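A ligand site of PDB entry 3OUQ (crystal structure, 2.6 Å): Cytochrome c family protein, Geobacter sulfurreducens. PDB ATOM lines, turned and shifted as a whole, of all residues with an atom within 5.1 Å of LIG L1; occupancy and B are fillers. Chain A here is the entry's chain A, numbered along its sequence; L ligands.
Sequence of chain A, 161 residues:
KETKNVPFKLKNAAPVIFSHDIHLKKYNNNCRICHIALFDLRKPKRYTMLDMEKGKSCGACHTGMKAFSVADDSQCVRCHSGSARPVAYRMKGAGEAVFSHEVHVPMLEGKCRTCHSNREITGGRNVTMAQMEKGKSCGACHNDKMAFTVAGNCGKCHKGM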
ATOM      1  N   VAL A   6     -12.946  -3.361  27.493  1.00  0.00           N
ATOM      2  CA  VAL A   6     -12.461  -4.589  26.852  1.00  0.00           C
ATOM      3  C   VAL A   6     -11.411  -5.292  27.714  1.00  0.00           C
ATOM      4  O   VAL A   6     -10.400  -4.692  28.075  1.00  0.00           O
ATOM      5  CB  VAL A   6     -11.845  -4.298  25.478  1.00  0.00           C
ATOM      6  CG1 VAL A   6     -11.565  -5.610  24.755  1.00  0.00           C
ATOM      7  CG2 VAL A   6     -12.786  -3.424  24.655  1.00  0.00           C
ATOM      8  N   PHE A   8      -8.421  -7.969  28.533  1.00  0.00           N
ATOM      9  CA  PHE A   8      -7.290  -8.640  27.903  1.00  0.00           C
ATOM     10  C   PHE A   8      -6.873  -9.717  28.910  1.00  0.00           C
ATOM     11  O   PHE A   8      -6.221  -9.426  29.904  1.00  0.00           O
ATOM     12  CB  PHE A   8      -6.146  -7.661  27.669  1.00  0.00           C
ATOM     13  CG  PHE A   8      -6.372  -6.743  26.514  1.00  0.00           C
ATOM     14  CD1 PHE A   8      -7.328  -5.727  26.582  1.00  0.00           C
ATOM     15  CD2 PHE A   8      -5.645  -6.893  25.345  1.00  0.00           C
ATOM     16  CE1 PHE A   8      -7.550  -4.876  25.498  1.00  0.00           C
ATOM     17  CE2 PHE A   8      -5.860  -6.058  24.256  1.00  0.00           C
ATOM     18  CZ  PHE A   8      -6.816  -5.042  24.324  1.00  0.00           C
ATOM     19  N   PHE A  18      -9.098  -2.513  29.158  1.00  0.00           N
ATOM     20  CA  PHE A  18      -9.051  -1.270  28.397  1.00  0.00           C
ATOM     21  C   PHE A  18     -10.419  -0.638  28.568  1.00  0.00           C
ATOM     22  O   PHE A  18     -11.445  -1.293  28.334  1.00  0.00           O
ATOM     23  CB  PHE A  18      -8.822  -1.525  26.913  1.00  0.00           C
ATOM     24  CG  PHE A  18      -9.022  -0.308  26.075  1.00  0.00           C
ATOM     25  CD1 PHE A  18      -8.032   0.672  25.994  1.00  0.00           C
ATOM     26  CD2 PHE A  18     -10.229  -0.092  25.414  1.00  0.00           C
ATOM     27  CE1 PHE A  18      -8.234   1.849  25.273  1.00  0.00           C
ATOM     28  CE2 PHE A  18     -10.436   1.077  24.693  1.00  0.00           C
ATOM     29  CZ  PHE A  18      -9.446   2.046  24.626  1.00  0.00           C
ATOM     30  N   HIS A  20     -12.895   2.304  27.287  1.00  0.00           N
ATOM     31  CA  HIS A  20     -13.170   3.300  26.249  1.00  0.00           C
ATOM     32  C   HIS A  20     -13.486   4.672  26.826  1.00  0.00           C
ATOM     33  O   HIS A  20     -12.999   5.683  26.332  1.00  0.00           O
ATOM     34  CB  HIS A  20     -14.362   2.869  25.388  1.00  0.00           C
ATOM     35  CG  HIS A  20     -14.010   1.900  24.296  1.00  0.00           C
ATOM     36  ND1 HIS A  20     -13.842   0.545  24.485  1.00  0.00           N
ATOM     37  CD2 HIS A  20     -13.782   2.112  22.983  1.00  0.00           C
ATOM     38  CE1 HIS A  20     -13.526   0.003  23.303  1.00  0.00           C
ATOM     39  NE2 HIS A  20     -13.471   0.913  22.352  1.00  0.00           N
ATOM     40  N   HIS A  23     -10.707   7.101  27.331  1.00  0.00           N
ATOM     41  CA  HIS A  23     -10.022   7.429  26.090  1.00  0.00           C
ATOM     42  C   HIS A  23     -10.891   8.305  25.194  1.00  0.00           C
ATOM     43  O   HIS A  23     -10.379   9.153  24.454  1.00  0.00           O
ATOM     44  CB  HIS A  23      -9.596   6.149  25.355  1.00  0.00           C
ATOM     45  CG  HIS A  23      -8.520   5.403  26.085  1.00  0.00           C
ATOM     46  ND1 HIS A  23      -8.754   4.528  27.119  1.00  0.00           N
ATOM     47  CD2 HIS A  23      -7.172   5.495  25.975  1.00  0.00           C
ATOM     48  CE1 HIS A  23      -7.560   4.150  27.596  1.00  0.00           C
ATOM     49  NE2 HIS A  23      -6.568   4.713  26.944  1.00  0.00           N
ATOM     50  N   LEU A  24     -12.209   8.114  25.283  1.00  0.00           N
ATOM     51  CA  LEU A  24     -13.148   8.920  24.509  1.00  0.00           C
ATOM     52  C   LEU A  24     -13.174  10.336  25.066  1.00  0.00           C
ATOM     53  O   LEU A  24     -13.110  11.295  24.312  1.00  0.00           O
ATOM     54  CB  LEU A  24     -14.552   8.306  24.560  1.00  0.00           C
ATOM     55  CG  LEU A  24     -14.659   6.917  23.952  1.00  0.00           C
ATOM     56  CD1 LEU A  24     -16.110   6.462  23.918  1.00  0.00           C
ATOM     57  CD2 LEU A  24     -14.077   6.939  22.554  1.00  0.00           C
ATOM     58  N   TYR A  27      -9.992  11.725  23.594  1.00  0.00           N
ATOM     59  CA  TYR A  27      -9.924  12.044  22.169  1.00  0.00           C
ATOM     60  C   TYR A  27     -11.217  12.610  21.593  1.00  0.00           C
ATOM     61  O   TYR A  27     -11.349  12.751  20.370  1.00  0.00           O
ATOM     62  CB  TYR A  27      -9.483  10.822  21.361  1.00  0.00           C
ATOM     63  CG  TYR A  27      -8.034  10.462  21.596  1.00  0.00           C
ATOM     64  CD1 TYR A  27      -7.675   9.590  22.623  1.00  0.00           C
ATOM     65  CD2 TYR A  27      -7.025  11.068  20.853  1.00  0.00           C
ATOM     66  CE1 TYR A  27      -6.334   9.315  22.899  1.00  0.00           C
ATOM     67  CE2 TYR A  27      -5.674  10.811  21.129  1.00  0.00           C
ATOM     68  CZ  TYR A  27      -5.345   9.932  22.158  1.00  0.00           C
ATOM     69  OH  TYR A  27      -4.029   9.708  22.468  1.00  0.00           O
ATOM     70  N   ASN A  29     -14.447  11.379  21.521  1.00  0.00           N
ATOM     71  CA  ASN A  29     -15.117  10.352  20.748  1.00  0.00           C
ATOM     72  C   ASN A  29     -14.570  10.108  19.357  1.00  0.00           C
ATOM     73  O   ASN A  29     -15.241   9.481  18.544  1.00  0.00           O
ATOM     74  CB  ASN A  29     -16.621  10.668  20.634  1.00  0.00           C
ATOM     75  CG  ASN A  29     -17.276  10.855  21.980  1.00  0.00           C
ATOM     76  OD1 ASN A  29     -17.057  11.865  22.650  1.00  0.00           O
ATOM     77  ND2 ASN A  29     -18.087   9.894  22.387  1.00  0.00           N
ATOM     78  N   ASN A  30     -13.367  10.581  19.045  1.00  0.00           N
ATOM     79  CA  ASN A  30     -12.848  10.332  17.710  1.00  0.00           C
ATOM     80  C   ASN A  30     -12.283   8.925  17.614  1.00  0.00           C
ATOM     81  O   ASN A  30     -11.089   8.705  17.795  1.00  0.00           O
ATOM     82  CB  ASN A  30     -11.776  11.344  17.326  1.00  0.00           C
ATOM     83  CG  ASN A  30     -11.293  11.157  15.900  1.00  0.00           C
ATOM     84  OD1 ASN A  30     -12.097  11.090  14.965  1.00  0.00           O
ATOM     85  ND2 ASN A  30      -9.978  11.081  15.721  1.00  0.00           N
ATOM     86  N   CYS A  31     -13.160   7.967  17.317  1.00  0.00           N
ATOM     87  CA  CYS A  31     -12.799   6.558  17.184  1.00  0.00           C
ATOM     88  C   CYS A  31     -11.703   6.290  16.167  1.00  0.00           C
ATOM     89  O   CYS A  31     -10.994   5.293  16.260  1.00  0.00           O
ATOM     90  CB  CYS A  31     -14.036   5.751  16.807  1.00  0.00           C
ATOM     91  SG  CYS A  31     -15.528   6.145  17.769  1.00  0.00           S
ATOM     92  N   ILE A  33      -8.873   7.562  15.802  1.00  0.00           N
ATOM     93  CA  ILE A  33      -7.520   7.558  16.366  1.00  0.00           C
ATOM     94  C   ILE A  33      -7.001   6.130  16.506  1.00  0.00           C
ATOM     95  O   ILE A  33      -5.916   5.802  16.028  1.00  0.00           O
ATOM     96  CB  ILE A  33      -7.462   8.210  17.767  1.00  0.00           C
ATOM     97  CG1 ILE A  33      -8.255   9.512  17.812  1.00  0.00           C
ATOM     98  CG2 ILE A  33      -6.012   8.463  18.129  1.00  0.00           C
ATOM     99  N   CYS A  34      -7.791   5.271  17.145  1.00  0.00           N
ATOM    100  CA  CYS A  34      -7.397   3.872  17.377  1.00  0.00           C
ATOM    101  C   CYS A  34      -8.005   2.772  16.491  1.00  0.00           C
ATOM    102  O   CYS A  34      -7.516   1.630  16.522  1.00  0.00           O
ATOM    103  CB  CYS A  34      -7.686   3.484  18.830  1.00  0.00           C
ATOM    104  SG  CYS A  34      -7.239   4.715  20.085  1.00  0.00           S
ATOM    105  N   HIS A  35      -9.054   3.078  15.721  1.00  0.00           N
ATOM    106  CA  HIS A  35      -9.670   2.020  14.930  1.00  0.00           C
ATOM    107  C   HIS A  35      -9.316   1.811  13.466  1.00  0.00           C
ATOM    108  O   HIS A  35      -9.432   2.670  12.589  1.00  0.00           O
ATOM    109  CB  HIS A  35     -11.184   2.023  15.113  1.00  0.00           C
ATOM    110  CG  HIS A  35     -11.635   1.408  16.413  1.00  0.00           C
ATOM    111  ND1 HIS A  35     -11.475   0.074  16.725  1.00  0.00           N
ATOM    112  CD2 HIS A  35     -12.162   1.971  17.520  1.00  0.00           C
ATOM    113  CE1 HIS A  35     -11.902  -0.109  17.997  1.00  0.00           C
ATOM    114  NE2 HIS A  35     -12.331   1.013  18.530  1.00  0.00           N
ATOM    115  N   LEU A  38      -4.514   1.295  14.690  1.00  0.00           N
ATOM    116  CA  LEU A  38      -3.792   0.776  15.842  1.00  0.00           C
ATOM    117  C   LEU A  38      -4.333  -0.630  16.076  1.00  0.00           C
ATOM    118  O   LEU A  38      -3.574  -1.612  16.107  1.00  0.00           O
ATOM    119  CB  LEU A  38      -4.076   1.645  17.067  1.00  0.00           C
ATOM    120  CG  LEU A  38      -3.815   3.144  16.966  1.00  0.00           C
ATOM    121  CD1 LEU A  38      -4.208   3.814  18.277  1.00  0.00           C
ATOM    122  CD2 LEU A  38      -2.341   3.420  16.661  1.00  0.00           C
ATOM    123  N   PHE A  39      -5.650  -0.738  16.233  1.00  0.00           N
ATOM    124  CA  PHE A  39      -6.275  -2.028  16.465  1.00  0.00           C
ATOM    125  C   PHE A  39      -7.155  -2.498  15.307  1.00  0.00           C
ATOM    126  O   PHE A  39      -8.227  -1.949  15.057  1.00  0.00           O
ATOM    127  CB  PHE A  39      -7.078  -1.978  17.762  1.00  0.00           C
ATOM    128  CG  PHE A  39      -6.270  -1.513  18.939  1.00  0.00           C
ATOM    129  CD1 PHE A  39      -5.971  -0.171  19.104  1.00  0.00           C
ATOM    130  CD2 PHE A  39      -5.804  -2.426  19.871  1.00  0.00           C
ATOM    131  CE1 PHE A  39      -5.200   0.253  20.181  1.00  0.00           C
ATOM    132  CE2 PHE A  39      -5.028  -2.004  20.962  1.00  0.00           C
ATOM    133  CZ  PHE A  39      -4.735  -0.660  21.113  1.00  0.00           C
ATOM    134  N   LEU A  41      -8.286  -5.467  15.277  1.00  0.00           N
ATOM    135  CA  LEU A  41      -9.279  -6.254  16.014  1.00  0.00           C
ATOM    136  C   LEU A  41      -9.904  -7.366  15.178  1.00  0.00           C
ATOM    137  O   LEU A  41     -11.094  -7.659  15.323  1.00  0.00           O
ATOM    138  CB  LEU A  41     -10.362  -5.306  16.542  1.00  0.00           C
ATOM    139  CG  LEU A  41     -11.581  -5.841  17.295  1.00  0.00           C
ATOM    140  CD1 LEU A  41     -11.180  -6.885  18.322  1.00  0.00           C
ATOM    141  CD2 LEU A  41     -12.287  -4.672  17.952  1.00  0.00           C
ATOM    142  N   PRO A  44      -5.836 -10.448  16.000  1.00  0.00           N
ATOM    143  CA  PRO A  44      -4.671  -9.995  16.760  1.00  0.00           C
ATOM    144  C   PRO A  44      -3.980 -11.098  17.542  1.00  0.00           C
ATOM    145  O   PRO A  44      -4.606 -12.081  17.972  1.00  0.00           O
ATOM    146  CB  PRO A  44      -5.264  -8.923  17.672  1.00  0.00           C
ATOM    147  CG  PRO A  44      -6.615  -9.496  18.001  1.00  0.00           C
ATOM    148  CD  PRO A  44      -7.096 -10.003  16.651  1.00  0.00           C
HETATM  149 FE1  LIG L   1     -12.728   0.982  20.446  1.00  0.00          FE
HETATM  150  C1  LIG L   1     -12.616  -2.401  20.929  1.00  0.00           C
HETATM  151  C2  LIG L   1     -16.008   0.731  19.437  1.00  0.00           C
HETATM  152  C3  LIG L   1     -12.955   4.421  20.278  1.00  0.00           C
HETATM  153  C4  LIG L   1      -9.449   1.261  21.329  1.00  0.00           C
HETATM  154  N1  LIG L   1     -14.022  -0.509  20.199  1.00  0.00           N
HETATM  155  C5  LIG L   1     -13.797  -1.860  20.428  1.00  0.00           C
HETATM  156  C6  LIG L   1     -14.986  -2.622  20.132  1.00  0.00           C
HETATM  157  C7  LIG L   1     -15.950  -1.762  19.716  1.00  0.00           C
HETATM  158  C8  LIG L   1     -15.335  -0.441  19.753  1.00  0.00           C
HETATM  159  C9  LIG L   1     -17.397  -2.107  19.376  1.00  0.00           C
HETATM  160  C10 LIG L   1     -15.151  -4.087  20.387  1.00  0.00           C
HETATM  161  C11 LIG L   1     -15.649  -4.362  21.786  1.00  0.00           C
HETATM  162  C12 LIG L   1     -15.435  -5.803  22.173  1.00  0.00           C
HETATM  163  O1  LIG L   1     -15.889  -6.685  21.417  1.00  0.00           O
HETATM  164  O2  LIG L   1     -14.813  -6.053  23.218  1.00  0.00           O
HETATM  165  N2  LIG L   1     -14.151   2.300  19.963  1.00  0.00           N
HETATM  166  C13 LIG L   1     -15.449   2.005  19.543  1.00  0.00           C
HETATM  167  C14 LIG L   1     -16.166   3.225  19.222  1.00  0.00           C
HETATM  168  C15 LIG L   1     -15.366   4.283  19.534  1.00  0.00           C
HETATM  169  C16 LIG L   1     -14.094   3.699  19.947  1.00  0.00           C
HETATM  170  C17 LIG L   1     -17.514   3.289  18.528  1.00  0.00           C
HETATM  171  C18 LIG L   1     -15.733   5.793  19.533  1.00  0.00           C
HETATM  172  C19 LIG L   1     -17.087   6.162  20.138  1.00  0.00           C
HETATM  173  N3  LIG L   1     -11.503   2.494  20.816  1.00  0.00           N
HETATM  174  C20 LIG L   1     -11.743   3.858  20.687  1.00  0.00           C
HETATM  175  C21 LIG L   1     -10.547   4.613  20.933  1.00  0.00           C
HETATM  176  C22 LIG L   1      -9.583   3.736  21.224  1.00  0.00           C
HETATM  177  C23 LIG L   1     -10.166   2.431  21.161  1.00  0.00           C
HETATM  178  C24 LIG L   1     -10.378   6.106  20.835  1.00  0.00           C
HETATM  179  C25 LIG L   1      -8.127   4.027  21.482  1.00  0.00           C
HETATM  180  C26 LIG L   1      -7.870   4.758  22.781  1.00  0.00           C
HETATM  181  N4  LIG L   1     -11.334  -0.284  20.972  1.00  0.00           N
HETATM  182  C27 LIG L   1     -10.002  -0.002  21.277  1.00  0.00           C
HETATM  183  C28 LIG L   1      -9.303  -1.181  21.766  1.00  0.00           C
HETATM  184  C29 LIG L   1     -10.205  -2.194  21.700  1.00  0.00           C
HETATM  185  C30 LIG L   1     -11.461  -1.657  21.197  1.00  0.00           C
HETATM  186  C31 LIG L   1      -7.905  -1.242  22.379  1.00  0.00           C
HETATM  187  C32 LIG L   1      -9.854  -3.621  22.044  1.00  0.00           C
HETATM  188  C33 LIG L   1      -9.701  -4.352  20.732  1.00  0.00           C
HETATM  189  C34 LIG L   1      -8.890  -5.609  20.888  1.00  0.00           C
HETATM  190  O3  LIG L   1      -9.199  -6.414  21.794  1.00  0.00           O
HETATM  191  O4  LIG L   1      -7.945  -5.795  20.081  1.00  0.00           O
HETATM  192 FE1  LG2 L   2      -4.562   4.652  27.221  1.00  0.00          FE
HETATM  193  C1  LG2 L   2      -4.962   6.821  29.863  1.00  0.00           C
HETATM  194  C2  LG2 L   2      -4.903   2.015  29.420  1.00  0.00           C
HETATM  195  C3  LG2 L   2      -4.267   2.396  24.628  1.00  0.00           C
HETATM  196  C4  LG2 L   2      -4.064   7.255  25.147  1.00  0.00           C
HETATM  197  N1  LG2 L   2      -4.864   4.479  29.191  1.00  0.00           N
HETATM  198  C5  LG2 L   2      -5.062   5.468  30.103  1.00  0.00           C
HETATM  199  C6  LG2 L   2      -5.341   4.953  31.416  1.00  0.00           C
HETATM  200  C7  LG2 L   2      -5.268   3.624  31.308  1.00  0.00           C
HETATM  201  C8  LG2 L   2      -4.972   3.314  29.935  1.00  0.00           C
HETATM  202  C9  LG2 L   2      -5.426   2.703  32.497  1.00  0.00           C
HETATM  203  C10 LG2 L   2      -5.548   5.747  32.706  1.00  0.00           C
HETATM  204  C11 LG2 L   2      -6.999   5.850  33.081  1.00  0.00           C
HETATM  205  C12 LG2 L   2      -7.216   6.671  34.318  1.00  0.00           C
HETATM  206  O1  LG2 L   2      -6.567   7.725  34.451  1.00  0.00           O
HETATM  207  O2  LG2 L   2      -8.048   6.281  35.167  1.00  0.00           O
HETATM  208  N2  LG2 L   2      -4.601   2.638  27.041  1.00  0.00           N
HETATM  209  C13 LG2 L   2      -4.747   1.692  28.067  1.00  0.00           C
HETATM  210  C14 LG2 L   2      -4.655   0.344  27.527  1.00  0.00           C
HETATM  211  C15 LG2 L   2      -4.457   0.434  26.190  1.00  0.00           C
HETATM  212  C16 LG2 L   2      -4.421   1.866  25.889  1.00  0.00           C
HETATM  213  C17 LG2 L   2      -4.712  -0.962  28.289  1.00  0.00           C
HETATM  214  C18 LG2 L   2      -4.185  -0.725  25.213  1.00  0.00           C
HETATM  215  C19 LG2 L   2      -5.066  -1.974  25.252  1.00  0.00           C
HETATM  216  N3  LG2 L   2      -4.309   4.776  25.300  1.00  0.00           N
HETATM  217  C20 LG2 L   2      -4.253   3.749  24.359  1.00  0.00           C
HETATM  218  C21 LG2 L   2      -4.043   4.291  23.017  1.00  0.00           C
HETATM  219  C22 LG2 L   2      -3.959   5.648  23.160  1.00  0.00           C
HETATM  220  C23 LG2 L   2      -4.119   5.953  24.580  1.00  0.00           C
HETATM  221  C24 LG2 L   2      -3.845   3.479  21.750  1.00  0.00           C
HETATM  222  C25 LG2 L   2      -3.557   6.669  22.116  1.00  0.00           C
HETATM  223  C26 LG2 L   2      -4.228   6.566  20.770  1.00  0.00           C
HETATM  224  N4  LG2 L   2      -4.491   6.618  27.487  1.00  0.00           N
HETATM  225  C27 LG2 L   2      -4.230   7.549  26.514  1.00  0.00           C
HETATM  226  C28 LG2 L   2      -4.298   8.886  27.097  1.00  0.00           C
HETATM  227  C29 LG2 L   2      -4.704   8.818  28.403  1.00  0.00           C
HETATM  228  C30 LG2 L   2      -4.730   7.367  28.636  1.00  0.00           C
HETATM  229  C31 LG2 L   2      -3.900  10.140  26.332  1.00  0.00           C
HETATM  230  C32 LG2 L   2      -5.357   9.953  29.225  1.00  0.00           C
HETATM  231  C33 LG2 L   2      -4.806  10.713  30.453  1.00  0.00           C
HETATM  232  C34 LG2 L   2      -4.977   9.967  31.791  1.00  0.00           C
HETATM  233  O3  LG2 L   2      -6.087   9.464  32.077  1.00  0.00           O
HETATM  234  O4  LG2 L   2      -3.988   9.901  32.570  1.00  0.00           O
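A carbon (C25) of LIG L1 is covalently linked to the side-chain sulfur (SG) of Cys 34.
SG of Cys 31 is covalently linked to C18 of LIG L1 (1.8 Å).
FE1 of LIG L1 is bound by NE2 of His 35, at 2.0 Å.
FE1 of LIG L1 is bound by NE2 of His 20 (2.0 Å).
An iron atom (FE1) of LG2 L2 is bound by a ring nitrogen (NE2) of His 23 (2.0 Å).
N of Phe 39 lies within hydrogen-bond range of O of Cys 34, at 3.0 Å.
The backbone carbonyl oxygen (O) of Phe 18 sits at hydrogen-bond distance from the backbone NH (N) of Val 6 (2.7 Å).
N of Asn 29 sits at hydrogen-bond distance from O of Leu 24, 3.1 Å away.
Val 6 touches LIG L1.
Phe 8 touches LIG L1.
CZ of Phe 18 touches C4 of LIG L1, 3.4 Å away.
His 23 touches LIG L1 (CD2 to C26, 3.4 Å).
Leu 24 touches LIG L1 (CD2 to C3, 3.6 Å).
O of Asn 29 touches C18 of LIG L1, 3.8 Å away.
Phe 39 touches LIG L1.
CD1 of Leu 41 touches C34 of LIG L1, at 3.7 Å.
Hydrophobic or aromatic side chains within 4 Å of LIG L1: Val 6, Phe 8, Phe 18, His 20, His 23, Leu 24, His 35, Phe 39 and Leu 41.
The nearest printed residue that does not touch LIG L1 is Asn 30 (4.1 Å).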
